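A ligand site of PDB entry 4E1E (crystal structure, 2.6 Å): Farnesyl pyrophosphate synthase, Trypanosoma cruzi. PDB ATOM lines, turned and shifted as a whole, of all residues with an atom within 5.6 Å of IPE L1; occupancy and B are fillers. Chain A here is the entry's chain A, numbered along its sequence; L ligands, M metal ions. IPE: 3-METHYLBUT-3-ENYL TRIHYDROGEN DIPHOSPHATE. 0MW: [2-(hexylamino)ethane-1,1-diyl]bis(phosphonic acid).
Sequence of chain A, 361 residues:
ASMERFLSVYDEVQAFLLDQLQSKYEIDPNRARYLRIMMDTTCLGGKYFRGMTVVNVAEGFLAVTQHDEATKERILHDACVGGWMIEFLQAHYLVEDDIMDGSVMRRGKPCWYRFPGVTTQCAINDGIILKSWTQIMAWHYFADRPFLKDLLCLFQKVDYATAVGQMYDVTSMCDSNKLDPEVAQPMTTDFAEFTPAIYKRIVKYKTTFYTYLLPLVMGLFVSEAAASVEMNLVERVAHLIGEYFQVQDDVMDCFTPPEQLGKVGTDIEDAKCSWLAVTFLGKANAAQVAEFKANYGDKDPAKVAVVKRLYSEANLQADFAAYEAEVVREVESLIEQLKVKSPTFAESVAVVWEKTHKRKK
O2B of IPE L1 lies within salt-bridge range of NH2 of Arg 107 (2.7 Å).
O1A of IPE L1 is in salt-bridge range of NH2 of Arg 50, at 2.8 Å.
The backbone NH (N) of Lys 47 is in hydrogen-bond range of an oxygen (O3B) of IPE L1 (3.2 Å).
NZ of Lys 47 is in salt-bridge range of O2A of IPE L1 (2.9 Å).
The side-chain amide nitrogen of Gln 90 is in hydrogen-bond range of an oxygen (O1A) of IPE L1.
NZ of Lys 263 lies within salt-bridge range of O3 of 0MW L2, at 3.1 Å.
NE2 of Gln 246 lies close to O5 of 0MW L2 (3.5 Å).
An oxygen (O3) of 0MW L2 lies within salt-bridge range of the guanidinium group (NH1) of Arg 106, at 2.7 Å.
NH2 of Arg 50 lies within hydrogen-bond range of OE1 of Gln 90.
The guanidinium group (NH1) of Arg 50 lies within hydrogen-bond range of the side-chain hydroxyl (OH) of Tyr 210 (3.5 Å).
The side-chain hydroxyl of Thr 211 lies within hydrogen-bond range of the guanidinium group of Arg 50 (2.8 Å).
NE2 of Gln 90 sits close to OH of Tyr 210.
The side-chain amino group (NZ) of Lys 263 is in salt-bridge range of the side-chain carboxylate (OD1) of Asp 249 (2.8 Å).
The backbone carbonyl oxygen (O) of Phe 245 sits at hydrogen-bond distance from the guanidinium group (NH1) of Arg 359 (3.2 Å).
NE2 of Gln 246 lies close to OD2 of Asp 249, 3.1 Å away.
The side-chain amide oxygen (OE1) of Gln 246 sits at hydrogen-bond distance from the side-chain hydroxyl (OG1) of Thr 207, 2.6 Å away.
Merely in contact with IPE L1: Gly 46 (3.6 Å), Tyr 210 (3.2 Å), Phe 245 (3.4 Å), Gln 246 (3.5 Å), Asp 249 (3.4 Å) and Lys 263 (3.3 Å).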
ATOM      1  N   GLY A  45      32.028 -29.074  26.610  1.00  0.00           N
ATOM      2  CA  GLY A  45      32.849 -27.928  26.226  1.00  0.00           C
ATOM      3  C   GLY A  45      31.997 -26.708  26.025  1.00  0.00           C
ATOM      4  O   GLY A  45      32.504 -25.578  26.042  1.00  0.00           O
ATOM      5  N   GLY A  46      30.695 -26.929  25.845  1.00  0.00           N
ATOM      6  CA  GLY A  46      29.737 -25.853  25.596  1.00  0.00           C
ATOM      7  C   GLY A  46      29.137 -25.289  26.872  1.00  0.00           C
ATOM      8  O   GLY A  46      29.533 -25.684  27.980  1.00  0.00           O
ATOM      9  N   LYS A  47      28.170 -24.389  26.700  1.00  0.00           N
ATOM     10  CA  LYS A  47      27.565 -23.634  27.796  1.00  0.00           C
ATOM     11  C   LYS A  47      26.551 -24.430  28.616  1.00  0.00           C
ATOM     12  O   LYS A  47      26.247 -24.047  29.747  1.00  0.00           O
ATOM     13  CB  LYS A  47      26.883 -22.382  27.254  1.00  0.00           C
ATOM     14  CG  LYS A  47      27.829 -21.269  26.842  1.00  0.00           C
ATOM     15  CD  LYS A  47      27.057 -19.997  26.484  1.00  0.00           C
ATOM     16  CE  LYS A  47      26.198 -20.172  25.237  1.00  0.00           C
ATOM     17  NZ  LYS A  47      27.034 -20.450  24.033  1.00  0.00           N
ATOM     18  N   TYR A  48      26.045 -25.506  28.024  1.00  0.00           N
ATOM     19  CA  TYR A  48      25.021 -26.387  28.627  1.00  0.00           C
ATOM     20  C   TYR A  48      23.727 -25.648  28.982  1.00  0.00           C
ATOM     21  O   TYR A  48      23.008 -26.044  29.896  1.00  0.00           O
ATOM     22  CB  TYR A  48      25.556 -27.133  29.860  1.00  0.00           C
ATOM     23  CG  TYR A  48      26.921 -27.794  29.703  1.00  0.00           C
ATOM     24  CD1 TYR A  48      28.027 -27.308  30.402  1.00  0.00           C
ATOM     25  CD2 TYR A  48      27.116 -28.892  28.859  1.00  0.00           C
ATOM     26  CE1 TYR A  48      29.276 -27.887  30.285  1.00  0.00           C
ATOM     27  CE2 TYR A  48      28.365 -29.482  28.729  1.00  0.00           C
ATOM     28  CZ  TYR A  48      29.443 -28.975  29.442  1.00  0.00           C
ATOM     29  OH  TYR A  48      30.692 -29.532  29.329  1.00  0.00           O
ATOM     30  N   PHE A  49      23.445 -24.566  28.244  1.00  0.00           N
ATOM     31  CA  PHE A  49      22.222 -23.789  28.448  1.00  0.00           C
ATOM     32  C   PHE A  49      20.965 -24.655  28.260  1.00  0.00           C
ATOM     33  O   PHE A  49      20.032 -24.568  29.061  1.00  0.00           O
ATOM     34  CB  PHE A  49      22.172 -22.569  27.513  1.00  0.00           C
ATOM     35  CG  PHE A  49      22.983 -21.386  28.002  1.00  0.00           C
ATOM     36  CD1 PHE A  49      23.894 -21.508  29.069  1.00  0.00           C
ATOM     37  CD2 PHE A  49      22.858 -20.148  27.367  1.00  0.00           C
ATOM     38  CE1 PHE A  49      24.650 -20.416  29.507  1.00  0.00           C
ATOM     39  CE2 PHE A  49      23.606 -19.037  27.805  1.00  0.00           C
ATOM     40  CZ  PHE A  49      24.500 -19.178  28.873  1.00  0.00           C
ATOM     41  N   ARG A  50      20.969 -25.479  27.224  1.00  0.00           N
ATOM     42  CA  ARG A  50      19.803 -26.299  26.885  1.00  0.00           C
ATOM     43  C   ARG A  50      19.540 -27.378  27.939  1.00  0.00           C
ATOM     44  O   ARG A  50      18.408 -27.547  28.403  1.00  0.00           O
ATOM     45  CB  ARG A  50      19.983 -26.925  25.495  1.00  0.00           C
ATOM     46  CG  ARG A  50      20.052 -25.908  24.379  1.00  0.00           C
ATOM     47  CD  ARG A  50      20.771 -26.474  23.177  1.00  0.00           C
ATOM     48  NE  ARG A  50      20.719 -25.575  22.023  1.00  0.00           N
ATOM     49  CZ  ARG A  50      21.656 -24.671  21.716  1.00  0.00           C
ATOM     50  NH1 ARG A  50      21.512 -23.907  20.645  1.00  0.00           N
ATOM     51  NH2 ARG A  50      22.740 -24.530  22.472  1.00  0.00           N
ATOM     52  N   GLU A  87      21.472 -32.135  24.693  1.00  0.00           N
ATOM     53  CA  GLU A  87      22.887 -31.808  24.487  1.00  0.00           C
ATOM     54  C   GLU A  87      23.522 -32.722  23.445  1.00  0.00           C
ATOM     55  O   GLU A  87      24.400 -32.299  22.692  1.00  0.00           O
ATOM     56  CB  GLU A  87      23.657 -31.854  25.814  1.00  0.00           C
ATOM     57  CG  GLU A  87      23.355 -30.712  26.784  1.00  0.00           C
ATOM     58  CD  GLU A  87      23.848 -29.349  26.294  1.00  0.00           C
ATOM     59  OE1 GLU A  87      24.913 -29.289  25.652  1.00  0.00           O
ATOM     60  OE2 GLU A  87      23.165 -28.341  26.560  1.00  0.00           O
ATOM     61  N   GLN A  90      22.235 -31.515  20.057  1.00  0.00           N
ATOM     62  CA  GLN A  90      23.033 -30.403  19.559  1.00  0.00           C
ATOM     63  C   GLN A  90      24.433 -30.815  19.116  1.00  0.00           C
ATOM     64  O   GLN A  90      24.972 -30.214  18.191  1.00  0.00           O
ATOM     65  CB  GLN A  90      23.145 -29.258  20.565  1.00  0.00           C
ATOM     66  CG  GLN A  90      23.308 -27.921  19.796  1.00  0.00           C
ATOM     67  CD  GLN A  90      24.190 -26.912  20.462  1.00  0.00           C
ATOM     68  OE1 GLN A  90      24.563 -27.065  21.623  1.00  0.00           O
ATOM     69  NE2 GLN A  90      24.553 -25.881  19.730  1.00  0.00           N
ATOM     70  N   LEU A  94      25.881 -29.676  15.510  1.00  0.00           N
ATOM     71  CA  LEU A  94      27.136 -28.960  15.332  1.00  0.00           C
ATOM     72  C   LEU A  94      28.136 -29.705  14.420  1.00  0.00           C
ATOM     73  O   LEU A  94      28.720 -29.105  13.503  1.00  0.00           O
ATOM     74  CB  LEU A  94      27.763 -28.621  16.682  1.00  0.00           C
ATOM     75  CG  LEU A  94      26.991 -27.701  17.633  1.00  0.00           C
ATOM     76  CD1 LEU A  94      27.945 -27.239  18.726  1.00  0.00           C
ATOM     77  CD2 LEU A  94      26.341 -26.504  16.931  1.00  0.00           C
ATOM     78  N   ARG A 106      35.646 -24.984  16.890  1.00  0.00           N
ATOM     79  CA  ARG A 106      34.389 -25.168  17.638  1.00  0.00           C
ATOM     80  C   ARG A 106      34.650 -25.504  19.106  1.00  0.00           C
ATOM     81  O   ARG A 106      35.391 -26.432  19.418  1.00  0.00           O
ATOM     82  CB  ARG A 106      33.510 -26.252  16.983  1.00  0.00           C
ATOM     83  CG  ARG A 106      32.306 -26.694  17.801  1.00  0.00           C
ATOM     84  CD  ARG A 106      31.168 -25.690  17.760  1.00  0.00           C
ATOM     85  NE  ARG A 106      30.425 -25.804  16.517  1.00  0.00           N
ATOM     86  CZ  ARG A 106      29.447 -24.990  16.129  1.00  0.00           C
ATOM     87  NH1 ARG A 106      29.065 -23.973  16.890  1.00  0.00           N
ATOM     88  NH2 ARG A 106      28.851 -25.192  14.957  1.00  0.00           N
ATOM     89  N   ARG A 107      34.018 -24.733  20.005  1.00  0.00           N
ATOM     90  CA  ARG A 107      34.260 -24.795  21.465  1.00  0.00           C
ATOM     91  C   ARG A 107      35.762 -24.756  21.790  1.00  0.00           C
ATOM     92  O   ARG A 107      36.259 -25.549  22.613  1.00  0.00           O
ATOM     93  CB  ARG A 107      33.589 -26.024  22.099  1.00  0.00           C
ATOM     94  CG  ARG A 107      32.060 -25.957  22.165  1.00  0.00           C
ATOM     95  CD  ARG A 107      31.482 -27.338  22.484  1.00  0.00           C
ATOM     96  NE  ARG A 107      30.024 -27.398  22.329  1.00  0.00           N
ATOM     97  CZ  ARG A 107      29.313 -28.527  22.334  1.00  0.00           C
ATOM     98  NH1 ARG A 107      29.944 -29.690  22.471  1.00  0.00           N
ATOM     99  NH2 ARG A 107      28.000 -28.502  22.200  1.00  0.00           N
ATOM    100  N   THR A 207      16.806 -22.727  14.929  1.00  0.00           N
ATOM    101  CA  THR A 207      17.289 -22.449  16.284  1.00  0.00           C
ATOM    102  C   THR A 207      16.248 -22.609  17.394  1.00  0.00           C
ATOM    103  O   THR A 207      16.483 -23.337  18.347  1.00  0.00           O
ATOM    104  CB  THR A 207      17.971 -21.026  16.392  1.00  0.00           C
ATOM    105  OG1 THR A 207      18.961 -20.875  15.368  1.00  0.00           O
ATOM    106  CG2 THR A 207      18.633 -20.823  17.768  1.00  0.00           C
ATOM    107  N   TYR A 210      14.700 -26.247  18.996  1.00  0.00           N
ATOM    108  CA  TYR A 210      15.607 -27.106  19.755  1.00  0.00           C
ATOM    109  C   TYR A 210      16.374 -26.429  20.890  1.00  0.00           C
ATOM    110  O   TYR A 210      16.831 -27.084  21.817  1.00  0.00           O
ATOM    111  CB  TYR A 210      16.520 -27.910  18.806  1.00  0.00           C
ATOM    112  CG  TYR A 210      17.889 -27.354  18.540  1.00  0.00           C
ATOM    113  CD1 TYR A 210      18.977 -27.722  19.324  1.00  0.00           C
ATOM    114  CD2 TYR A 210      18.115 -26.476  17.471  1.00  0.00           C
ATOM    115  CE1 TYR A 210      20.251 -27.228  19.085  1.00  0.00           C
ATOM    116  CE2 TYR A 210      19.397 -25.978  17.213  1.00  0.00           C
ATOM    117  CZ  TYR A 210      20.452 -26.359  18.025  1.00  0.00           C
ATOM    118  OH  TYR A 210      21.714 -25.891  17.809  1.00  0.00           O
ATOM    119  N   THR A 211      16.512 -25.099  20.825  1.00  0.00           N
ATOM    120  CA  THR A 211      17.298 -24.352  21.814  1.00  0.00           C
ATOM    121  C   THR A 211      16.428 -23.829  22.945  1.00  0.00           C
ATOM    122  O   THR A 211      16.918 -23.587  24.055  1.00  0.00           O
ATOM    123  CB  THR A 211      18.065 -23.169  21.149  1.00  0.00           C
ATOM    124  OG1 THR A 211      18.829 -23.661  20.033  1.00  0.00           O
ATOM    125  CG2 THR A 211      19.000 -22.500  22.125  1.00  0.00           C
ATOM    126  N   PHE A 245      18.568 -15.009  20.539  1.00  0.00           N
ATOM    127  CA  PHE A 245      19.758 -15.846  20.717  1.00  0.00           C
ATOM    128  C   PHE A 245      20.495 -16.006  19.390  1.00  0.00           C
ATOM    129  O   PHE A 245      21.723 -15.994  19.350  1.00  0.00           O
ATOM    130  CB  PHE A 245      19.377 -17.225  21.286  1.00  0.00           C
ATOM    131  CG  PHE A 245      20.543 -18.171  21.437  1.00  0.00           C
ATOM    132  CD1 PHE A 245      20.918 -19.022  20.403  1.00  0.00           C
ATOM    133  CD2 PHE A 245      21.249 -18.247  22.632  1.00  0.00           C
ATOM    134  CE1 PHE A 245      21.979 -19.904  20.541  1.00  0.00           C
ATOM    135  CE2 PHE A 245      22.318 -19.137  22.784  1.00  0.00           C
ATOM    136  CZ  PHE A 245      22.686 -19.959  21.740  1.00  0.00           C
ATOM    137  N   GLN A 246      19.722 -16.162  18.315  1.00  0.00           N
ATOM    138  CA  GLN A 246      20.316 -16.328  16.992  1.00  0.00           C
ATOM    139  C   GLN A 246      20.823 -15.003  16.458  1.00  0.00           C
ATOM    140  O   GLN A 246      21.918 -14.951  15.860  1.00  0.00           O
ATOM    141  CB  GLN A 246      19.319 -16.969  16.017  1.00  0.00           C
ATOM    142  CG  GLN A 246      19.922 -17.306  14.658  1.00  0.00           C
ATOM    143  CD  GLN A 246      21.103 -18.257  14.737  1.00  0.00           C
ATOM    144  OE1 GLN A 246      21.054 -19.275  15.431  1.00  0.00           O
ATOM    145  NE2 GLN A 246      22.188 -17.929  14.037  1.00  0.00           N
ATOM    146  N   ASP A 249      24.034 -14.589  18.099  1.00  0.00           N
ATOM    147  CA  ASP A 249      25.026 -15.484  17.478  1.00  0.00           C
ATOM    148  C   ASP A 249      25.536 -14.881  16.177  1.00  0.00           C
ATOM    149  O   ASP A 249      26.733 -14.964  15.877  1.00  0.00           O
ATOM    150  CB  ASP A 249      24.395 -16.867  17.233  1.00  0.00           C
ATOM    151  CG  ASP A 249      25.292 -17.818  16.419  1.00  0.00           C
ATOM    152  OD1 ASP A 249      26.236 -18.415  16.971  1.00  0.00           O
ATOM    153  OD2 ASP A 249      25.005 -18.008  15.218  1.00  0.00           O
ATOM    154  N   LYS A 263      34.751 -19.783  18.166  1.00  0.00           N
ATOM    155  CA  LYS A 263      34.700 -20.355  16.829  1.00  0.00           C
ATOM    156  C   LYS A 263      35.052 -19.225  15.865  1.00  0.00           C
ATOM    157  O   LYS A 263      35.049 -18.054  16.264  1.00  0.00           O
ATOM    158  CB  LYS A 263      33.327 -20.990  16.529  1.00  0.00           C
ATOM    159  CG  LYS A 263      32.156 -20.010  16.547  1.00  0.00           C
ATOM    160  CD  LYS A 263      30.856 -20.652  17.037  1.00  0.00           C
ATOM    161  CE  LYS A 263      29.652 -19.769  16.706  1.00  0.00           C
ATOM    162  NZ  LYS A 263      28.371 -20.194  17.328  1.00  0.00           N
ATOM    163  N   ARG A 359      24.798 -13.266  27.829  1.00  0.00           N
ATOM    164  CA  ARG A 359      25.833 -14.163  27.293  1.00  0.00           C
ATOM    165  C   ARG A 359      26.758 -13.397  26.341  1.00  0.00           C
ATOM    166  O   ARG A 359      26.338 -12.415  25.725  1.00  0.00           O
ATOM    167  CB  ARG A 359      25.224 -15.383  26.600  1.00  0.00           C
ATOM    168  CG  ARG A 359      24.777 -15.169  25.153  1.00  0.00           C
ATOM    169  CD  ARG A 359      23.981 -16.377  24.678  1.00  0.00           C
ATOM    170  NE  ARG A 359      23.738 -16.391  23.239  1.00  0.00           N
ATOM    171  CZ  ARG A 359      24.588 -16.841  22.321  1.00  0.00           C
ATOM    172  NH1 ARG A 359      24.251 -16.827  21.043  1.00  0.00           N
ATOM    173  NH2 ARG A 359      25.776 -17.317  22.690  1.00  0.00           N
ATOM    174  N   LYS A 361      29.408 -15.541  24.724  1.00  0.00           N
ATOM    175  CA  LYS A 361      30.228 -16.680  24.275  1.00  0.00           C
ATOM    176  C   LYS A 361      29.400 -17.712  23.496  1.00  0.00           C
ATOM    177  O   LYS A 361      28.201 -17.860  23.714  1.00  0.00           O
ATOM    178  CB  LYS A 361      30.903 -17.323  25.497  1.00  0.00           C
ATOM    179  CG  LYS A 361      31.811 -18.518  25.231  1.00  0.00           C
ATOM    180  CD  LYS A 361      32.377 -19.032  26.559  1.00  0.00           C
ATOM    181  CE  LYS A 361      33.023 -20.412  26.426  1.00  0.00           C
ATOM    182  NZ  LYS A 361      34.440 -20.340  25.959  1.00  0.00           N
HETATM  183  C1  IPE L   1      25.848 -21.262  19.236  1.00  0.00           C
HETATM  184  O1  IPE L   1      26.153 -21.548  20.621  1.00  0.00           O
HETATM  185  C2  IPE L   1      25.162 -22.418  18.498  1.00  0.00           C
HETATM  186  C3  IPE L   1      23.825 -21.989  17.892  1.00  0.00           C
HETATM  187  C4  IPE L   1      22.862 -22.870  17.729  1.00  0.00           C
HETATM  188  C5  IPE L   1      23.568 -20.575  17.439  1.00  0.00           C
HETATM  189  PA  IPE L   1      25.354 -22.665  21.459  1.00  0.00           P
HETATM  190  O1A IPE L   1      24.233 -23.129  20.580  1.00  0.00           O
HETATM  191  O2A IPE L   1      25.025 -22.146  22.834  1.00  0.00           O
HETATM  192  O3A IPE L   1      26.416 -23.885  21.554  1.00  0.00           O
HETATM  193  PB  IPE L   1      27.151 -24.501  22.850  1.00  0.00           P
HETATM  194  O1B IPE L   1      28.556 -23.959  22.740  1.00  0.00           O
HETATM  195  O2B IPE L   1      27.078 -25.973  22.578  1.00  0.00           O
HETATM  196  O3B IPE L   1      26.389 -24.039  24.083  1.00  0.00           O
HETATM  197  O1  0MW L   2      27.986 -22.462  13.422  1.00  0.00           O
HETATM  198  P1  0MW L   2      26.963 -21.932  14.399  1.00  0.00           P
HETATM  199  O2  0MW L   2      26.827 -20.435  14.397  1.00  0.00           O
HETATM  200  O3  0MW L   2      27.103 -22.539  15.770  1.00  0.00           O
HETATM  201  C9  0MW L   2      25.413 -22.617  13.728  1.00  0.00           C
HETATM  202  P2  0MW L   2      24.732 -21.410  12.552  1.00  0.00           P
HETATM  203  O5  0MW L   2      24.807 -20.060  13.190  1.00  0.00           O
HETATM  204  O4  0MW L   2      25.697 -21.577  11.399  1.00  0.00           O
HETATM  205  O6  0MW L   2      23.306 -21.806  12.268  1.00  0.00           O
HETATM  206  C8  0MW L   2      24.458 -23.001  14.861  1.00  0.00           C
HETATM  207  N1  0MW L   2      23.113 -23.399  14.392  1.00  0.00           N
HETATM  208  C7  0MW L   2      22.998 -24.853  14.259  1.00  0.00           C
HETATM  209  C6  0MW L   2      22.186 -25.160  13.011  1.00  0.00           C
HETATM  210  C5  0MW L   2      21.361 -26.433  13.152  1.00  0.00           C
HETATM  211  C4  0MW L   2      22.111 -27.563  12.476  1.00  0.00           C
HETATM  212  C3  0MW L   2      21.185 -28.653  11.943  1.00  0.00           C
HETATM  213  C2  0MW L   2      21.983 -29.656  11.155  1.00  0.00           C
HETATM  214 MG    MG M   1      26.214 -18.401  13.396  1.00  0.00          MG
